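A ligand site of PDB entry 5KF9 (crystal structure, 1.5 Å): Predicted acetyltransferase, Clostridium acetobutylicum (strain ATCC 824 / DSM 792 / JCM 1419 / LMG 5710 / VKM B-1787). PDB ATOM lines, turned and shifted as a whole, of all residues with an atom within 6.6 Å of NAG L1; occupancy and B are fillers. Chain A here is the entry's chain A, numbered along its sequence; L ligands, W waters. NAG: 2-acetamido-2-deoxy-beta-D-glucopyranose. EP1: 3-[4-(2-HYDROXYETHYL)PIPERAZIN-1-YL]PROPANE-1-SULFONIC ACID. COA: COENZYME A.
The guanidinium group (NH1) of Arg 192 lies within hydrogen-bond range of a ring nitrogen (ND1) of His 120 (3.1 Å).
The side-chain carboxylate (OE2) of Glu 196 lies within salt-bridge range of the guanidinium group (NE) of Arg 192 (2.7 Å).
The backbone nitrogen of Pro 252 sits close to an oxygen (O3) of NAG L1, 3.2 Å away.
Merely in contact with NAG L1: Gly 251, Tyr 297, Ile 286, Pro 235 and Thr 289.
Within 4 Å of NAG L1: Arg 192, Trp 193, Glu 196, Pro 235, Gly 251, Pro 252, Ile 253, Ile 286, Asp 287, Trp 288, Thr 289 and Tyr 297.
The nearest printed residue that does not touch NAG L1 is His 120 (4.6 Å).
NE1 of Trp 193 sits at hydrogen-bond distance from O6 of NAG L1 (3.0 Å).
O3 of NAG L1 sits at hydrogen-bond distance from OD1 of Asp 287, at 2.6 Å.
O of Asp 287 lies within hydrogen-bond range of N2 of NAG L1 (3.0 Å).
The guanidinium group (NE) of Arg 192 is in hydrogen-bond range of an oxygen (O6) of NAG L1 (3.5 Å).
N of Trp 193 lies within hydrogen-bond range of O2S of EP1 L2 (2.8 Å).
N of Ile 253 sits at hydrogen-bond distance from O7 of NAG L1.
An oxygen (O3S) of EP1 L2 is in hydrogen-bond range of the backbone NH (N) of Arg 192, at 3.2 Å.
The backbone carbonyl oxygen (O) of Trp 288 lies within hydrogen-bond range of a nitrogen (N2) of NAG L1 (3.4 Å).
O of Trp 288 sits at hydrogen-bond distance from O8 of EP1 L2, at 2.7 Å.
An oxygen (O6) of NAG L1 is in hydrogen-bond range of the side-chain carboxylate (OE2) of Glu 196.
Water W1 bridges O4 of NAG L1 (2.7 Å) and OE1 of Glu 196 (3.0 Å).
Water W2 lies within hydrogen-bond range of O of Ile 253 (2.7 Å), O7 of NAG L1 (2.8 Å) and N4P of COA L3 (2.9 Å).
An oxygen (O1) of NAG L1 lies within hydrogen-bond range of an oxygen (O8) of EP1 L2.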
ATOM      1  N   HIS A 120     -26.061 -17.372  34.492  1.00  0.00           N
ATOM      2  CA  HIS A 120     -24.860 -17.087  35.294  1.00  0.00           C
ATOM      3  C   HIS A 120     -23.934 -16.157  34.574  1.00  0.00           C
ATOM      4  O   HIS A 120     -23.959 -16.080  33.349  1.00  0.00           O
ATOM      5  CB  HIS A 120     -24.105 -18.389  35.608  1.00  0.00           C
ATOM      6  CG  HIS A 120     -23.601 -19.086  34.390  1.00  0.00           C
ATOM      7  ND1 HIS A 120     -24.450 -19.672  33.485  1.00  0.00           N
ATOM      8  CD2 HIS A 120     -22.346 -19.252  33.895  1.00  0.00           C
ATOM      9  CE1 HIS A 120     -23.751 -20.205  32.494  1.00  0.00           C
ATOM     10  NE2 HIS A 120     -22.470 -19.952  32.716  1.00  0.00           N
ATOM     11  N   ARG A 192     -31.391 -28.814  32.521  1.00  0.00           N
ATOM     12  CA  ARG A 192     -30.990 -27.453  32.212  1.00  0.00           C
ATOM     13  C   ARG A 192     -30.838 -27.177  30.727  1.00  0.00           C
ATOM     14  O   ARG A 192     -31.194 -26.113  30.243  1.00  0.00           O
ATOM     15  CB  ARG A 192     -29.658 -27.132  32.918  1.00  0.00           C
ATOM     16  CG  ARG A 192     -29.219 -25.710  32.665  1.00  0.00           C
ATOM     17  CD  ARG A 192     -28.022 -25.292  33.521  1.00  0.00           C
ATOM     18  NE  ARG A 192     -27.574 -23.962  33.154  1.00  0.00           N
ATOM     19  CZ  ARG A 192     -27.003 -23.080  33.991  1.00  0.00           C
ATOM     20  NH1 ARG A 192     -26.639 -21.893  33.550  1.00  0.00           N
ATOM     21  NH2 ARG A 192     -26.917 -23.369  35.263  1.00  0.00           N
ATOM     22  N   TRP A 193     -30.319 -28.165  30.004  1.00  0.00           N
ATOM     23  CA  TRP A 193     -30.107 -27.921  28.595  1.00  0.00           C
ATOM     24  C   TRP A 193     -31.407 -27.813  27.850  1.00  0.00           C
ATOM     25  O   TRP A 193     -31.478 -27.023  26.921  1.00  0.00           O
ATOM     26  CB  TRP A 193     -29.204 -28.980  28.022  1.00  0.00           C
ATOM     27  CG  TRP A 193     -27.750 -28.839  28.446  1.00  0.00           C
ATOM     28  CD1 TRP A 193     -27.200 -27.859  29.198  1.00  0.00           C
ATOM     29  CD2 TRP A 193     -26.687 -29.675  28.032  1.00  0.00           C
ATOM     30  NE1 TRP A 193     -25.844 -28.097  29.355  1.00  0.00           N
ATOM     31  CE2 TRP A 193     -25.505 -29.205  28.638  1.00  0.00           C
ATOM     32  CE3 TRP A 193     -26.620 -30.843  27.270  1.00  0.00           C
ATOM     33  CZ2 TRP A 193     -24.278 -29.848  28.491  1.00  0.00           C
ATOM     34  CZ3 TRP A 193     -25.391 -31.460  27.108  1.00  0.00           C
ATOM     35  CH2 TRP A 193     -24.240 -30.944  27.675  1.00  0.00           C
ATOM     36  N   GLU A 196     -32.628 -24.384  28.607  1.00  0.00           N
ATOM     37  CA  GLU A 196     -31.854 -23.421  27.870  1.00  0.00           C
ATOM     38  C   GLU A 196     -32.314 -23.307  26.410  1.00  0.00           C
ATOM     39  O   GLU A 196     -32.432 -22.197  25.904  1.00  0.00           O
ATOM     40  CB  GLU A 196     -30.338 -23.731  28.008  1.00  0.00           C
ATOM     41  CG  GLU A 196     -29.691 -23.368  29.342  1.00  0.00           C
ATOM     42  CD  GLU A 196     -28.208 -23.793  29.375  1.00  0.00           C
ATOM     43  OE1 GLU A 196     -27.630 -24.164  28.322  1.00  0.00           O
ATOM     44  OE2 GLU A 196     -27.622 -23.721  30.470  1.00  0.00           O
ATOM     45  N   PHE A 200     -33.493 -19.869  25.191  1.00  0.00           N
ATOM     46  CA  PHE A 200     -32.587 -19.151  24.345  1.00  0.00           C
ATOM     47  C   PHE A 200     -33.265 -18.853  23.011  1.00  0.00           C
ATOM     48  O   PHE A 200     -33.034 -17.798  22.439  1.00  0.00           O
ATOM     49  CB  PHE A 200     -31.247 -19.856  24.123  1.00  0.00           C
ATOM     50  CG  PHE A 200     -30.385 -19.968  25.361  1.00  0.00           C
ATOM     51  CD1 PHE A 200     -30.724 -19.358  26.545  1.00  0.00           C
ATOM     52  CD2 PHE A 200     -29.265 -20.758  25.302  1.00  0.00           C
ATOM     53  CE1 PHE A 200     -29.910 -19.470  27.677  1.00  0.00           C
ATOM     54  CE2 PHE A 200     -28.455 -20.863  26.413  1.00  0.00           C
ATOM     55  CZ  PHE A 200     -28.801 -20.245  27.605  1.00  0.00           C
ATOM     56  N   PRO A 235     -22.844 -18.177  27.072  1.00  0.00           N
ATOM     57  CA  PRO A 235     -21.640 -18.234  27.869  1.00  0.00           C
ATOM     58  C   PRO A 235     -20.311 -18.300  27.135  1.00  0.00           C
ATOM     59  O   PRO A 235     -19.339 -17.643  27.500  1.00  0.00           O
ATOM     60  CB  PRO A 235     -21.898 -19.454  28.781  1.00  0.00           C
ATOM     61  CG  PRO A 235     -23.347 -19.555  28.887  1.00  0.00           C
ATOM     62  CD  PRO A 235     -23.897 -19.080  27.562  1.00  0.00           C
ATOM     63  N   PRO A 236     -20.219 -19.096  26.036  1.00  0.00           N
ATOM     64  CA  PRO A 236     -18.904 -19.100  25.346  1.00  0.00           C
ATOM     65  C   PRO A 236     -18.432 -17.730  24.852  1.00  0.00           C
ATOM     66  O   PRO A 236     -17.241 -17.492  24.680  1.00  0.00           O
ATOM     67  CB  PRO A 236     -19.174 -20.011  24.141  1.00  0.00           C
ATOM     68  CG  PRO A 236     -20.285 -20.902  24.590  1.00  0.00           C
ATOM     69  CD  PRO A 236     -21.175 -20.058  25.469  1.00  0.00           C
ATOM     70  N   LEU A 250     -18.421 -22.503  21.393  1.00  0.00           N
ATOM     71  CA  LEU A 250     -19.149 -23.721  21.289  1.00  0.00           C
ATOM     72  C   LEU A 250     -19.559 -24.163  22.659  1.00  0.00           C
ATOM     73  O   LEU A 250     -18.729 -24.116  23.582  1.00  0.00           O
ATOM     74  CB  LEU A 250     -18.330 -24.759  20.507  1.00  0.00           C
ATOM     75  CG  LEU A 250     -18.992 -26.101  20.230  1.00  0.00           C
ATOM     76  CD1 LEU A 250     -18.355 -26.668  18.964  1.00  0.00           C
ATOM     77  CD2 LEU A 250     -18.794 -27.016  21.406  1.00  0.00           C
ATOM     78  N   GLY A 251     -20.803 -24.558  22.823  1.00  0.00           N
ATOM     79  CA  GLY A 251     -21.218 -25.330  24.009  1.00  0.00           C
ATOM     80  C   GLY A 251     -22.593 -24.916  24.317  1.00  0.00           C
ATOM     81  O   GLY A 251     -22.935 -23.739  24.128  1.00  0.00           O
ATOM     82  N   PRO A 252     -23.410 -25.864  24.795  1.00  0.00           N
ATOM     83  CA  PRO A 252     -23.151 -27.253  25.090  1.00  0.00           C
ATOM     84  C   PRO A 252     -23.065 -28.155  23.865  1.00  0.00           C
ATOM     85  O   PRO A 252     -23.347 -27.697  22.746  1.00  0.00           O
ATOM     86  CB  PRO A 252     -24.378 -27.684  25.863  1.00  0.00           C
ATOM     87  CG  PRO A 252     -25.412 -26.670  25.649  1.00  0.00           C
ATOM     88  CD  PRO A 252     -24.721 -25.408  25.263  1.00  0.00           C
ATOM     89  N   ILE A 253     -22.682 -29.384  24.099  1.00  0.00           N
ATOM     90  CA  ILE A 253     -22.505 -30.456  23.121  1.00  0.00           C
ATOM     91  C   ILE A 253     -22.870 -31.774  23.782  1.00  0.00           C
ATOM     92  O   ILE A 253     -22.435 -32.074  24.892  1.00  0.00           O
ATOM     93  CB  ILE A 253     -21.115 -30.468  22.462  1.00  0.00           C
ATOM     94  CG1 ILE A 253     -21.016 -31.590  21.428  1.00  0.00           C
ATOM     95  CG2 ILE A 253     -20.046 -30.537  23.555  1.00  0.00           C
ATOM     96  CD1 ILE A 253     -19.811 -31.425  20.559  1.00  0.00           C
ATOM     97  N   GLY A 254     -23.755 -32.534  23.168  1.00  0.00           N
ATOM     98  CA  GLY A 254     -24.229 -33.762  23.781  1.00  0.00           C
ATOM     99  C   GLY A 254     -24.630 -34.784  22.738  1.00  0.00           C
ATOM    100  O   GLY A 254     -25.167 -34.425  21.702  1.00  0.00           O
ATOM    101  N   ILE A 286     -14.861 -22.707  24.590  1.00  0.00           N
ATOM    102  CA  ILE A 286     -15.713 -23.806  24.985  1.00  0.00           C
ATOM    103  C   ILE A 286     -15.903 -23.613  26.471  1.00  0.00           C
ATOM    104  O   ILE A 286     -14.933 -23.764  27.232  1.00  0.00           O
ATOM    105  CB  ILE A 286     -15.151 -25.156  24.566  1.00  0.00           C
ATOM    106  CG1 ILE A 286     -15.022 -25.180  23.007  1.00  0.00           C
ATOM    107  CG2 ILE A 286     -16.058 -26.246  25.107  1.00  0.00           C
ATOM    108  CD1 ILE A 286     -14.526 -26.474  22.396  1.00  0.00           C
ATOM    109  N   ASP A 287     -17.100 -23.364  26.932  1.00  0.00           N
ATOM    110  CA  ASP A 287     -17.271 -22.914  28.328  1.00  0.00           C
ATOM    111  C   ASP A 287     -17.601 -24.075  29.244  1.00  0.00           C
ATOM    112  O   ASP A 287     -18.223 -25.064  28.856  1.00  0.00           O
ATOM    113  CB  ASP A 287     -18.404 -21.879  28.411  1.00  0.00           C
ATOM    114  CG  ASP A 287     -19.770 -22.457  28.192  1.00  0.00           C
ATOM    115  OD1 ASP A 287     -19.989 -23.041  27.083  1.00  0.00           O
ATOM    116  OD2 ASP A 287     -20.652 -22.445  29.129  1.00  0.00           O
ATOM    117  N   TRP A 288     -17.243 -23.891  30.533  1.00  0.00           N
ATOM    118  CA  TRP A 288     -17.746 -24.698  31.649  1.00  0.00           C
ATOM    119  C   TRP A 288     -17.583 -26.197  31.354  1.00  0.00           C
ATOM    120  O   TRP A 288     -18.550 -26.961  31.286  1.00  0.00           O
ATOM    121  CB  TRP A 288     -19.177 -24.347  31.983  1.00  0.00           C
ATOM    122  CG  TRP A 288     -19.703 -24.789  33.330  1.00  0.00           C
ATOM    123  CD1 TRP A 288     -19.179 -25.735  34.162  1.00  0.00           C
ATOM    124  CD2 TRP A 288     -20.907 -24.325  33.937  1.00  0.00           C
ATOM    125  NE1 TRP A 288     -19.978 -25.848  35.268  1.00  0.00           N
ATOM    126  CE2 TRP A 288     -21.079 -25.049  35.129  1.00  0.00           C
ATOM    127  CE3 TRP A 288     -21.874 -23.390  33.577  1.00  0.00           C
ATOM    128  CZ2 TRP A 288     -22.141 -24.833  35.991  1.00  0.00           C
ATOM    129  CZ3 TRP A 288     -22.966 -23.214  34.416  1.00  0.00           C
ATOM    130  CH2 TRP A 288     -23.083 -23.910  35.606  1.00  0.00           C
ATOM    131  N   THR A 289     -16.315 -26.612  31.323  1.00  0.00           N
ATOM    132  CA  THR A 289     -15.937 -28.006  31.117  1.00  0.00           C
ATOM    133  C   THR A 289     -15.373 -28.591  32.435  1.00  0.00           C
ATOM    134  O   THR A 289     -14.915 -27.878  33.283  1.00  0.00           O
ATOM    135  CB  THR A 289     -14.913 -28.208  30.024  1.00  0.00           C
ATOM    136  OG1 THR A 289     -13.630 -27.683  30.403  1.00  0.00           O
ATOM    137  CG2 THR A 289     -15.362 -27.559  28.734  1.00  0.00           C
ATOM    138  N   ILE A 293     -12.896 -34.140  30.786  1.00  0.00           N
ATOM    139  CA  ILE A 293     -13.244 -34.017  29.371  1.00  0.00           C
ATOM    140  C   ILE A 293     -12.345 -33.072  28.599  1.00  0.00           C
ATOM    141  O   ILE A 293     -12.438 -32.952  27.362  1.00  0.00           O
ATOM    142  CB  ILE A 293     -14.749 -33.649  29.136  1.00  0.00           C
ATOM    143  CG1 ILE A 293     -15.214 -34.061  27.706  1.00  0.00           C
ATOM    144  CG2 ILE A 293     -14.981 -32.178  29.408  1.00  0.00           C
ATOM    145  CD1 ILE A 293     -15.180 -35.557  27.434  1.00  0.00           C
ATOM    146  N   TYR A 297     -11.526 -32.032  23.873  1.00  0.00           N
ATOM    147  CA  TYR A 297     -11.378 -30.803  23.152  1.00  0.00           C
ATOM    148  C   TYR A 297      -9.912 -30.479  22.843  1.00  0.00           C
ATOM    149  O   TYR A 297      -9.586 -29.813  21.877  1.00  0.00           O
ATOM    150  CB  TYR A 297     -12.027 -29.665  23.952  1.00  0.00           C
ATOM    151  CG  TYR A 297     -13.450 -29.899  24.315  1.00  0.00           C
ATOM    152  CD1 TYR A 297     -14.456 -29.768  23.360  1.00  0.00           C
ATOM    153  CD2 TYR A 297     -13.831 -30.300  25.585  1.00  0.00           C
ATOM    154  CE1 TYR A 297     -15.764 -30.041  23.654  1.00  0.00           C
ATOM    155  CE2 TYR A 297     -15.162 -30.534  25.889  1.00  0.00           C
ATOM    156  CZ  TYR A 297     -16.102 -30.361  24.928  1.00  0.00           C
ATOM    157  OH  TYR A 297     -17.417 -30.640  25.245  1.00  0.00           O
HETATM  158  C1  NAG L   1     -21.920 -27.160  30.359  1.00  0.00           C
HETATM  159  C2  NAG L   1     -21.617 -26.815  28.917  1.00  0.00           C
HETATM  160  C3  NAG L   1     -21.800 -25.315  28.735  1.00  0.00           C
HETATM  161  C4  NAG L   1     -23.141 -24.780  29.263  1.00  0.00           C
HETATM  162  C5  NAG L   1     -23.294 -25.281  30.690  1.00  0.00           C
HETATM  163  C6  NAG L   1     -24.575 -24.888  31.384  1.00  0.00           C
HETATM  164  C7  NAG L   1     -20.151 -28.133  27.477  1.00  0.00           C
HETATM  165  C8  NAG L   1     -18.805 -28.169  26.812  1.00  0.00           C
HETATM  166  N2  NAG L   1     -20.318 -27.213  28.450  1.00  0.00           N
HETATM  167  O1  NAG L   1     -21.857 -28.565  30.538  1.00  0.00           O
HETATM  168  O3  NAG L   1     -21.684 -25.037  27.335  1.00  0.00           O
HETATM  169  O4  NAG L   1     -23.130 -23.350  29.199  1.00  0.00           O
HETATM  170  O5  NAG L   1     -23.217 -26.692  30.659  1.00  0.00           O
HETATM  171  O6  NAG L   1     -25.697 -25.451  30.663  1.00  0.00           O
HETATM  172  O7  NAG L   1     -21.007 -28.922  27.053  1.00  0.00           O
HETATM  173  O2S EP1 L   2     -29.706 -30.791  30.609  1.00  0.00           O
HETATM  174  S   EP1 L   2     -29.210 -31.757  31.533  1.00  0.00           S
HETATM  175  O3S EP1 L   2     -29.242 -31.159  32.843  1.00  0.00           O
HETATM  176  O1S EP1 L   2     -30.261 -33.020  31.552  1.00  0.00           O
HETATM  177  C11 EP1 L   2     -27.689 -32.300  31.168  1.00  0.00           C
HETATM  178  C10 EP1 L   2     -26.682 -31.551  32.026  1.00  0.00           C
HETATM  179  C9  EP1 L   2     -25.263 -31.959  31.667  1.00  0.00           C
HETATM  180  N1  EP1 L   2     -24.228 -30.979  32.083  1.00  0.00           N
HETATM  181  C2  EP1 L   2     -24.643 -29.741  32.789  1.00  0.00           C
HETATM  182  C3  EP1 L   2     -23.498 -28.792  33.158  1.00  0.00           C
HETATM  183  N4  EP1 L   2     -22.239 -29.508  33.490  1.00  0.00           N
HETATM  184  C5  EP1 L   2     -21.934 -30.787  32.833  1.00  0.00           C
HETATM  185  C6  EP1 L   2     -23.154 -31.690  32.770  1.00  0.00           C
HETATM  186  C7  EP1 L   2     -21.111 -28.610  33.798  1.00  0.00           C
HETATM  187  C8  EP1 L   2     -19.727 -29.211  33.631  1.00  0.00           C
HETATM  188  O8  EP1 L   2     -19.438 -29.326  32.240  1.00  0.00           O
HETATM  189  O5B COA L   3     -16.316 -39.299  20.147  1.00  0.00           O
HETATM  190  P1A COA L   3     -16.351 -40.037  21.553  1.00  0.00           P
HETATM  191  O1A COA L   3     -14.955 -39.813  22.056  1.00  0.00           O
HETATM  192  O2A COA L   3     -16.793 -41.468  21.498  1.00  0.00           O
HETATM  193  O3A COA L   3     -17.244 -39.390  22.753  1.00  0.00           O
HETATM  194  P2A COA L   3     -18.791 -39.587  22.965  1.00  0.00           P
HETATM  195  O4A COA L   3     -19.017 -40.306  24.260  1.00  0.00           O
HETATM  196  O5A COA L   3     -19.584 -39.899  21.698  1.00  0.00           O
HETATM  197  O6A COA L   3     -19.075 -38.002  23.085  1.00  0.00           O
HETATM  198  CBP COA L   3     -19.558 -36.312  24.651  1.00  0.00           C
HETATM  199  CCP COA L   3     -18.474 -37.180  24.084  1.00  0.00           C
HETATM  200  CDP COA L   3     -20.352 -35.740  23.496  1.00  0.00           C
HETATM  201  CEP COA L   3     -19.063 -35.070  25.349  1.00  0.00           C
HETATM  202  CAP COA L   3     -20.552 -37.225  25.375  1.00  0.00           C
HETATM  203  OAP COA L   3     -19.956 -38.035  26.400  1.00  0.00           O
HETATM  204  C9P COA L   3     -21.764 -36.602  25.993  1.00  0.00           C
HETATM  205  O9P COA L   3     -22.781 -36.252  25.393  1.00  0.00           O
HETATM  206  N8P COA L   3     -21.772 -36.534  27.329  1.00  0.00           N
HETATM  207  C7P COA L   3     -22.964 -36.109  28.035  1.00  0.00           C
HETATM  208  C6P COA L   3     -22.911 -34.611  28.278  1.00  0.00           C
HETATM  209  C5P COA L   3     -22.010 -34.395  29.479  1.00  0.00           C
HETATM  210  O5P COA L   3     -22.238 -34.902  30.589  1.00  0.00           O
HETATM  211  N4P COA L   3     -20.970 -33.606  29.239  1.00  0.00           N
HETATM  212  O   HOH W   1     -25.253 -22.495  27.709  1.00  0.00           O
HETATM  213  O   HOH W   2     -20.792 -31.707  27.022  1.00  0.00           O
